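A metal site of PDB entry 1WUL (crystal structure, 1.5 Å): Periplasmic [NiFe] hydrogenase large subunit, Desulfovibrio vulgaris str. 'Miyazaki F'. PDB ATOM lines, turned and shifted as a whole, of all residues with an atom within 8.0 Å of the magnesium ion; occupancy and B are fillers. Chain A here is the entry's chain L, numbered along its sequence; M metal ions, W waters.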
ATOM      1  N   PHE A  40      -2.620 -24.129 -29.127  1.00  0.00           N
ATOM      2  CA  PHE A  40      -3.501 -24.635 -28.074  1.00  0.00           C
ATOM      3  C   PHE A  40      -3.164 -26.109 -27.811  1.00  0.00           C
ATOM      4  O   PHE A  40      -2.945 -26.850 -28.800  1.00  0.00           O
ATOM      5  CB  PHE A  40      -4.957 -24.525 -28.481  1.00  0.00           C
ATOM      6  CG  PHE A  40      -5.967 -25.115 -27.503  1.00  0.00           C
ATOM      7  CD1 PHE A  40      -6.329 -24.409 -26.363  1.00  0.00           C
ATOM      8  CD2 PHE A  40      -6.545 -26.356 -27.757  1.00  0.00           C
ATOM      9  CE1 PHE A  40      -7.276 -24.936 -25.489  1.00  0.00           C
ATOM     10  CE2 PHE A  40      -7.502 -26.855 -26.894  1.00  0.00           C
ATOM     11  CZ  PHE A  40      -7.905 -26.149 -25.772  1.00  0.00           C
ATOM     12  N   GLU A  44      -6.603 -28.424 -19.647  1.00  0.00           N
ATOM     13  CA  GLU A  44      -7.791 -28.434 -18.796  1.00  0.00           C
ATOM     14  C   GLU A  44      -8.818 -29.471 -19.249  1.00  0.00           C
ATOM     15  O   GLU A  44      -9.521 -30.099 -18.439  1.00  0.00           O
ATOM     16  CB  GLU A  44      -8.434 -27.028 -18.765  1.00  0.00           C
ATOM     17  CG  GLU A  44      -7.520 -25.984 -18.095  1.00  0.00           C
ATOM     18  CD  GLU A  44      -7.786 -24.562 -18.570  1.00  0.00           C
ATOM     19  OE1 GLU A  44      -8.307 -24.411 -19.703  1.00  0.00           O
ATOM     20  OE2 GLU A  44      -7.440 -23.601 -17.828  1.00  0.00           O
ATOM     21  N   GLU A 319     -12.482 -14.819 -16.723  1.00  0.00           N
ATOM     22  CA  GLU A 319     -11.747 -15.003 -17.984  1.00  0.00           C
ATOM     23  C   GLU A 319     -12.688 -14.852 -19.164  1.00  0.00           C
ATOM     24  O   GLU A 319     -13.622 -15.651 -19.273  1.00  0.00           O
ATOM     25  CB  GLU A 319     -11.049 -16.369 -18.038  1.00  0.00           C
ATOM     26  CG  GLU A 319      -9.952 -16.442 -16.962  1.00  0.00           C
ATOM     27  CD  GLU A 319      -9.222 -17.777 -17.174  1.00  0.00           C
ATOM     28  OE1 GLU A 319      -8.083 -17.707 -17.679  1.00  0.00           O
ATOM     29  OE2 GLU A 319      -9.735 -18.863 -16.856  1.00  0.00           O
ATOM     30  N   TYR A 326     -12.699 -19.500 -28.494  1.00  0.00           N
ATOM     31  CA  TYR A 326     -13.562 -20.398 -27.742  1.00  0.00           C
ATOM     32  C   TYR A 326     -15.003 -20.047 -28.030  1.00  0.00           C
ATOM     33  O   TYR A 326     -15.312 -18.993 -28.583  1.00  0.00           O
ATOM     34  CB  TYR A 326     -13.320 -20.313 -26.211  1.00  0.00           C
ATOM     35  CG  TYR A 326     -11.880 -20.652 -25.910  1.00  0.00           C
ATOM     36  CD1 TYR A 326     -10.925 -19.638 -25.806  1.00  0.00           C
ATOM     37  CD2 TYR A 326     -11.466 -21.978 -25.751  1.00  0.00           C
ATOM     38  CE1 TYR A 326      -9.593 -19.945 -25.527  1.00  0.00           C
ATOM     39  CE2 TYR A 326     -10.106 -22.271 -25.489  1.00  0.00           C
ATOM     40  CZ  TYR A 326      -9.167 -21.264 -25.372  1.00  0.00           C
ATOM     41  OH  TYR A 326      -7.840 -21.553 -25.124  1.00  0.00           O
ATOM     42  N   PRO A 334     -12.981 -18.856 -12.701  1.00  0.00           N
ATOM     43  CA  PRO A 334     -12.383 -20.171 -12.924  1.00  0.00           C
ATOM     44  C   PRO A 334     -13.019 -21.334 -12.175  1.00  0.00           C
ATOM     45  O   PRO A 334     -12.833 -22.442 -12.691  1.00  0.00           O
ATOM     46  CB  PRO A 334     -10.912 -20.043 -12.465  1.00  0.00           C
ATOM     47  CG  PRO A 334     -10.711 -18.628 -12.193  1.00  0.00           C
ATOM     48  CD  PRO A 334     -12.003 -17.869 -12.269  1.00  0.00           C
ATOM     49  N   GLY A 337     -15.198 -22.271 -14.794  1.00  0.00           N
ATOM     50  CA  GLY A 337     -14.536 -22.098 -16.076  1.00  0.00           C
ATOM     51  C   GLY A 337     -15.033 -23.055 -17.143  1.00  0.00           C
ATOM     52  O   GLY A 337     -15.596 -24.135 -16.879  1.00  0.00           O
ATOM     53  N   GLN A 338     -14.786 -22.637 -18.389  1.00  0.00           N
ATOM     54  CA  GLN A 338     -15.114 -23.429 -19.558  1.00  0.00           C
ATOM     55  C   GLN A 338     -13.949 -23.358 -20.542  1.00  0.00           C
ATOM     56  O   GLN A 338     -13.448 -22.236 -20.692  1.00  0.00           O
ATOM     57  CB  GLN A 338     -16.352 -22.915 -20.303  1.00  0.00           C
ATOM     58  CG  GLN A 338     -17.595 -22.907 -19.417  1.00  0.00           C
ATOM     59  CD  GLN A 338     -18.814 -22.429 -20.182  1.00  0.00           C
ATOM     60  OE1 GLN A 338     -19.770 -23.195 -20.305  1.00  0.00           O
ATOM     61  NE2 GLN A 338     -18.776 -21.196 -20.644  1.00  0.00           N
ATOM     62  N   THR A 339     -13.645 -24.498 -21.145  1.00  0.00           N
ATOM     63  CA  THR A 339     -12.580 -24.506 -22.168  1.00  0.00           C
ATOM     64  C   THR A 339     -13.085 -25.281 -23.381  1.00  0.00           C
ATOM     65  O   THR A 339     -12.969 -26.508 -23.495  1.00  0.00           O
ATOM     66  CB  THR A 339     -11.288 -25.068 -21.586  1.00  0.00           C
ATOM     67  OG1 THR A 339     -10.963 -24.298 -20.389  1.00  0.00           O
ATOM     68  CG2 THR A 339     -10.145 -24.907 -22.574  1.00  0.00           C
ATOM     69  N   TRP A 354      -5.552 -17.939 -28.815  1.00  0.00           N
ATOM     70  CA  TRP A 354      -5.951 -19.097 -28.012  1.00  0.00           C
ATOM     71  C   TRP A 354      -5.906 -18.768 -26.535  1.00  0.00           C
ATOM     72  O   TRP A 354      -6.336 -19.555 -25.688  1.00  0.00           O
ATOM     73  CB  TRP A 354      -5.037 -20.294 -28.326  1.00  0.00           C
ATOM     74  CG  TRP A 354      -5.331 -20.962 -29.635  1.00  0.00           C
ATOM     75  CD1 TRP A 354      -4.518 -20.994 -30.732  1.00  0.00           C
ATOM     76  CD2 TRP A 354      -6.527 -21.709 -29.987  1.00  0.00           C
ATOM     77  NE1 TRP A 354      -5.136 -21.705 -31.739  1.00  0.00           N
ATOM     78  CE2 TRP A 354      -6.366 -22.157 -31.303  1.00  0.00           C
ATOM     79  CE3 TRP A 354      -7.697 -22.013 -29.283  1.00  0.00           C
ATOM     80  CZ2 TRP A 354      -7.366 -22.906 -31.934  1.00  0.00           C
ATOM     81  CZ3 TRP A 354      -8.694 -22.758 -29.879  1.00  0.00           C
ATOM     82  CH2 TRP A 354      -8.496 -23.199 -31.221  1.00  0.00           C
ATOM     83  N   MET A 355      -5.362 -17.596 -26.154  1.00  0.00           N
ATOM     84  CA  MET A 355      -5.461 -17.235 -24.748  1.00  0.00           C
ATOM     85  C   MET A 355      -6.832 -16.656 -24.436  1.00  0.00           C
ATOM     86  O   MET A 355      -7.387 -15.893 -25.235  1.00  0.00           O
ATOM     87  CB  MET A 355      -4.431 -16.166 -24.377  1.00  0.00           C
ATOM     88  CG  MET A 355      -2.997 -16.679 -24.301  1.00  0.00           C
ATOM     89  SD  MET A 355      -2.023 -15.486 -23.364  1.00  0.00           S
ATOM     90  CE  MET A 355      -0.331 -15.892 -23.876  1.00  0.00           C
ATOM     91  N   LYS A 356      -7.363 -16.990 -23.247  1.00  0.00           N
ATOM     92  CA  LYS A 356      -8.476 -16.260 -22.656  1.00  0.00           C
ATOM     93  C   LYS A 356      -7.984 -14.905 -22.163  1.00  0.00           C
ATOM     94  O   LYS A 356      -6.755 -14.690 -22.132  1.00  0.00           O
ATOM     95  CB  LYS A 356      -9.070 -17.049 -21.493  1.00  0.00           C
ATOM     96  CG  LYS A 356      -9.607 -18.434 -21.878  1.00  0.00           C
ATOM     97  CD  LYS A 356     -10.146 -19.180 -20.671  1.00  0.00           C
ATOM     98  CE  LYS A 356     -10.756 -20.523 -21.037  1.00  0.00           C
ATOM     99  NZ  LYS A 356     -10.909 -21.404 -19.836  1.00  0.00           N
ATOM    100  N   PRO A 358      -8.121 -12.722 -18.967  1.00  0.00           N
ATOM    101  CA  PRO A 358      -8.535 -12.541 -17.571  1.00  0.00           C
ATOM    102  C   PRO A 358      -8.687 -11.052 -17.268  1.00  0.00           C
ATOM    103  O   PRO A 358      -7.881 -10.214 -17.723  1.00  0.00           O
ATOM    104  CB  PRO A 358      -7.358 -13.110 -16.798  1.00  0.00           C
ATOM    105  CG  PRO A 358      -6.580 -13.948 -17.774  1.00  0.00           C
ATOM    106  CD  PRO A 358      -6.732 -13.190 -19.082  1.00  0.00           C
ATOM    107  N   SER A 465      -2.710 -19.163 -10.751  1.00  0.00           N
ATOM    108  CA  SER A 465      -3.699 -19.803  -9.873  1.00  0.00           C
ATOM    109  C   SER A 465      -4.243 -21.038 -10.579  1.00  0.00           C
ATOM    110  O   SER A 465      -4.485 -21.004 -11.797  1.00  0.00           O
ATOM    111  CB  SER A 465      -4.788 -18.808  -9.455  1.00  0.00           C
ATOM    112  OG  SER A 465      -5.416 -18.133 -10.537  1.00  0.00           O
ATOM    113  N   TRP A 467      -7.326 -23.964 -10.119  1.00  0.00           N
ATOM    114  CA  TRP A 467      -8.628 -24.012  -9.483  1.00  0.00           C
ATOM    115  C   TRP A 467      -9.259 -25.372  -9.727  1.00  0.00           C
ATOM    116  O   TRP A 467      -9.402 -25.769 -10.871  1.00  0.00           O
ATOM    117  CB  TRP A 467      -9.519 -22.921 -10.104  1.00  0.00           C
ATOM    118  CG  TRP A 467      -8.953 -21.539 -10.063  1.00  0.00           C
ATOM    119  CD1 TRP A 467      -7.969 -20.973 -10.812  1.00  0.00           C
ATOM    120  CD2 TRP A 467      -9.391 -20.521  -9.143  1.00  0.00           C
ATOM    121  NE1 TRP A 467      -7.770 -19.667 -10.428  1.00  0.00           N
ATOM    122  CE2 TRP A 467      -8.634 -19.370  -9.394  1.00  0.00           C
ATOM    123  CE3 TRP A 467     -10.356 -20.483  -8.125  1.00  0.00           C
ATOM    124  CZ2 TRP A 467      -8.827 -18.187  -8.666  1.00  0.00           C
ATOM    125  CZ3 TRP A 467     -10.548 -19.322  -7.401  1.00  0.00           C
ATOM    126  CH2 TRP A 467      -9.788 -18.194  -7.677  1.00  0.00           C
ATOM    127  N   PHE A 478     -11.034 -28.315 -13.827  1.00  0.00           N
ATOM    128  CA  PHE A 478      -9.698 -27.888 -13.427  1.00  0.00           C
ATOM    129  C   PHE A 478      -9.360 -26.712 -14.343  1.00  0.00           C
ATOM    130  O   PHE A 478      -9.335 -26.921 -15.565  1.00  0.00           O
ATOM    131  CB  PHE A 478      -8.662 -28.997 -13.524  1.00  0.00           C
ATOM    132  CG  PHE A 478      -7.421 -28.687 -12.677  1.00  0.00           C
ATOM    133  CD1 PHE A 478      -6.511 -27.699 -13.034  1.00  0.00           C
ATOM    134  CD2 PHE A 478      -7.215 -29.367 -11.498  1.00  0.00           C
ATOM    135  CE1 PHE A 478      -5.407 -27.419 -12.233  1.00  0.00           C
ATOM    136  CE2 PHE A 478      -6.105 -29.164 -10.698  1.00  0.00           C
ATOM    137  CZ  PHE A 478      -5.186 -28.147 -11.056  1.00  0.00           C
ATOM    138  N   GLN A 479      -9.137 -25.552 -13.764  1.00  0.00           N
ATOM    139  CA  GLN A 479      -8.825 -24.362 -14.578  1.00  0.00           C
ATOM    140  C   GLN A 479      -7.502 -23.757 -14.129  1.00  0.00           C
ATOM    141  O   GLN A 479      -7.304 -23.577 -12.911  1.00  0.00           O
ATOM    142  CB  GLN A 479      -9.967 -23.333 -14.489  1.00  0.00           C
ATOM    143  CG  GLN A 479     -11.268 -23.876 -15.062  1.00  0.00           C
ATOM    144  CD  GLN A 479     -11.233 -23.948 -16.576  1.00  0.00           C
ATOM    145  OE1 GLN A 479     -10.617 -23.098 -17.249  1.00  0.00           O
ATOM    146  NE2 GLN A 479     -11.930 -24.959 -17.096  1.00  0.00           N
ATOM    147  N   LEU A 480      -6.647 -23.467 -15.123  1.00  0.00           N
ATOM    148  CA  LEU A 480      -5.434 -22.705 -14.883  1.00  0.00           C
ATOM    149  C   LEU A 480      -5.643 -21.276 -15.375  1.00  0.00           C
ATOM    150  O   LEU A 480      -6.178 -21.097 -16.466  1.00  0.00           O
ATOM    151  CB  LEU A 480      -4.227 -23.279 -15.614  1.00  0.00           C
ATOM    152  CG  LEU A 480      -3.740 -24.692 -15.271  1.00  0.00           C
ATOM    153  CD1 LEU A 480      -4.724 -25.761 -15.677  1.00  0.00           C
ATOM    154  CD2 LEU A 480      -2.388 -24.937 -15.952  1.00  0.00           C
ATOM    155  N   VAL A 481      -5.242 -20.295 -14.593  1.00  0.00           N
ATOM    156  CA  VAL A 481      -5.258 -18.881 -14.934  1.00  0.00           C
ATOM    157  C   VAL A 481      -3.792 -18.471 -14.680  1.00  0.00           C
ATOM    158  O   VAL A 481      -3.297 -18.488 -13.543  1.00  0.00           O
ATOM    159  CB  VAL A 481      -6.223 -18.047 -14.099  1.00  0.00           C
ATOM    160  CG1 VAL A 481      -6.252 -16.604 -14.629  1.00  0.00           C
ATOM    161  CG2 VAL A 481      -7.640 -18.621 -14.095  1.00  0.00           C
ATOM    162  N   VAL A 482      -3.094 -18.202 -15.783  1.00  0.00           N
ATOM    163  CA  VAL A 482      -1.615 -18.179 -15.685  1.00  0.00           C
ATOM    164  C   VAL A 482      -1.114 -16.765 -15.879  1.00  0.00           C
ATOM    165  O   VAL A 482      -1.804 -15.976 -16.534  1.00  0.00           O
ATOM    166  CB  VAL A 482      -1.086 -19.188 -16.729  1.00  0.00           C
ATOM    167  CG1 VAL A 482       0.402 -19.413 -16.675  1.00  0.00           C
ATOM    168  CG2 VAL A 482      -1.725 -20.563 -16.535  1.00  0.00           C
ATOM    169  N   THR A 485      -1.355 -15.322 -19.238  1.00  0.00           N
ATOM    170  CA  THR A 485      -2.732 -15.162 -19.700  1.00  0.00           C
ATOM    171  C   THR A 485      -3.203 -13.749 -19.344  1.00  0.00           C
ATOM    172  O   THR A 485      -3.795 -13.041 -20.159  1.00  0.00           O
ATOM    173  CB  THR A 485      -3.705 -16.157 -19.039  1.00  0.00           C
ATOM    174  OG1 THR A 485      -3.101 -17.451 -18.932  1.00  0.00           O
ATOM    175  CG2 THR A 485      -4.988 -16.237 -19.838  1.00  0.00           C
ATOM    176  N   CYS A 531       2.373 -21.434 -21.180  1.00  0.00           N
ATOM    177  CA  CYS A 531       1.707 -21.010 -19.942  1.00  0.00           C
ATOM    178  C   CYS A 531       0.395 -20.294 -20.213  1.00  0.00           C
ATOM    179  O   CYS A 531      -0.651 -20.594 -19.620  1.00  0.00           O
ATOM    180  CB  CYS A 531       2.607 -20.034 -19.157  1.00  0.00           C
ATOM    181  SG  CYS A 531       3.618 -20.930 -17.965  1.00  0.00           S
ATOM    182  N   GLY A 532       0.412 -19.275 -21.082  1.00  0.00           N
ATOM    183  CA  GLY A 532      -0.786 -18.446 -21.212  1.00  0.00           C
ATOM    184  C   GLY A 532      -1.990 -19.229 -21.720  1.00  0.00           C
ATOM    185  O   GLY A 532      -3.113 -18.932 -21.293  1.00  0.00           O
ATOM    186  N   VAL A 533      -1.727 -20.202 -22.621  1.00  0.00           N
ATOM    187  CA  VAL A 533      -2.810 -20.929 -23.286  1.00  0.00           C
ATOM    188  C   VAL A 533      -3.112 -22.284 -22.688  1.00  0.00           C
ATOM    189  O   VAL A 533      -4.289 -22.686 -22.487  1.00  0.00           O
ATOM    190  CB  VAL A 533      -2.526 -21.230 -24.786  1.00  0.00           C
ATOM    191  CG1 VAL A 533      -3.661 -22.039 -25.412  1.00  0.00           C
ATOM    192  CG2 VAL A 533      -2.239 -19.937 -25.547  1.00  0.00           C
ATOM    193  N   HIS A 534      -2.058 -23.075 -22.315  1.00  0.00           N
ATOM    194  CA  HIS A 534      -2.200 -24.426 -21.756  1.00  0.00           C
ATOM    195  C   HIS A 534      -3.217 -25.249 -22.554  1.00  0.00           C
ATOM    196  O   HIS A 534      -3.122 -25.162 -23.810  1.00  0.00           O
ATOM    197  CB  HIS A 534      -2.466 -24.500 -20.230  1.00  0.00           C
ATOM    198  CG  HIS A 534      -3.421 -23.451 -19.718  1.00  0.00           C
ATOM    199  ND1 HIS A 534      -3.013 -22.123 -19.547  1.00  0.00           N
ATOM    200  CD2 HIS A 534      -4.726 -23.461 -19.410  1.00  0.00           C
ATOM    201  CE1 HIS A 534      -4.023 -21.381 -19.129  1.00  0.00           C
ATOM    202  NE2 HIS A 534      -5.070 -22.173 -19.043  1.00  0.00           N
ATOM    203  OXT HIS A 534      -4.027 -25.975 -22.090  1.00  0.00           O
HETATM  204 MG    MG M   1      -7.042 -21.609 -18.305  1.00  0.00          MG
HETATM  205  O   HOH W   1      -6.657 -19.582 -18.837  1.00  0.00           O
HETATM  206  O   HOH W   2      -8.862 -21.101 -17.576  1.00  0.00           O
HETATM  207  O   HOH W   3      -7.932 -21.898 -20.159  1.00  0.00           O
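OE2 of Glu 44 sits close to OE1 of Gln 479.
The side-chain carboxylate of Glu 44 is in hydrogen-bond range of the side-chain hydroxyl of Thr 339.
The side-chain carboxylate of Glu 44 is in salt-bridge range of the side-chain amino group of Lys 356 (3.98 Å).
The backbone carbonyl oxygen of Cys 531 sits at hydrogen-bond distance from a ring nitrogen (ND1) of His 534, at 2.8 Å.
Three residues have an atom within 4 Å of the magnesium ion: Glu 44, Leu 480 and His 534.
The magnesium ion is bound by water W2 (2.0 Å), water W3 (2.1 Å), OE2 of Glu 44 (2.1 Å), O of Leu 480 (2.1 Å), water W1 (2.1 Å) and NE2 of His 534 (2.2 Å).
Water W3 lies within hydrogen-bond range of OE1 of Glu 44 and NZ of Lys 356.
Water W2 lies within hydrogen-bond range of the side-chain carboxylate of Glu 319 (2.5 Å), the side-chain amide oxygen of Gln 479 (2.7 Å) and the side-chain amino group of Lys 356 (3.1 Å).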
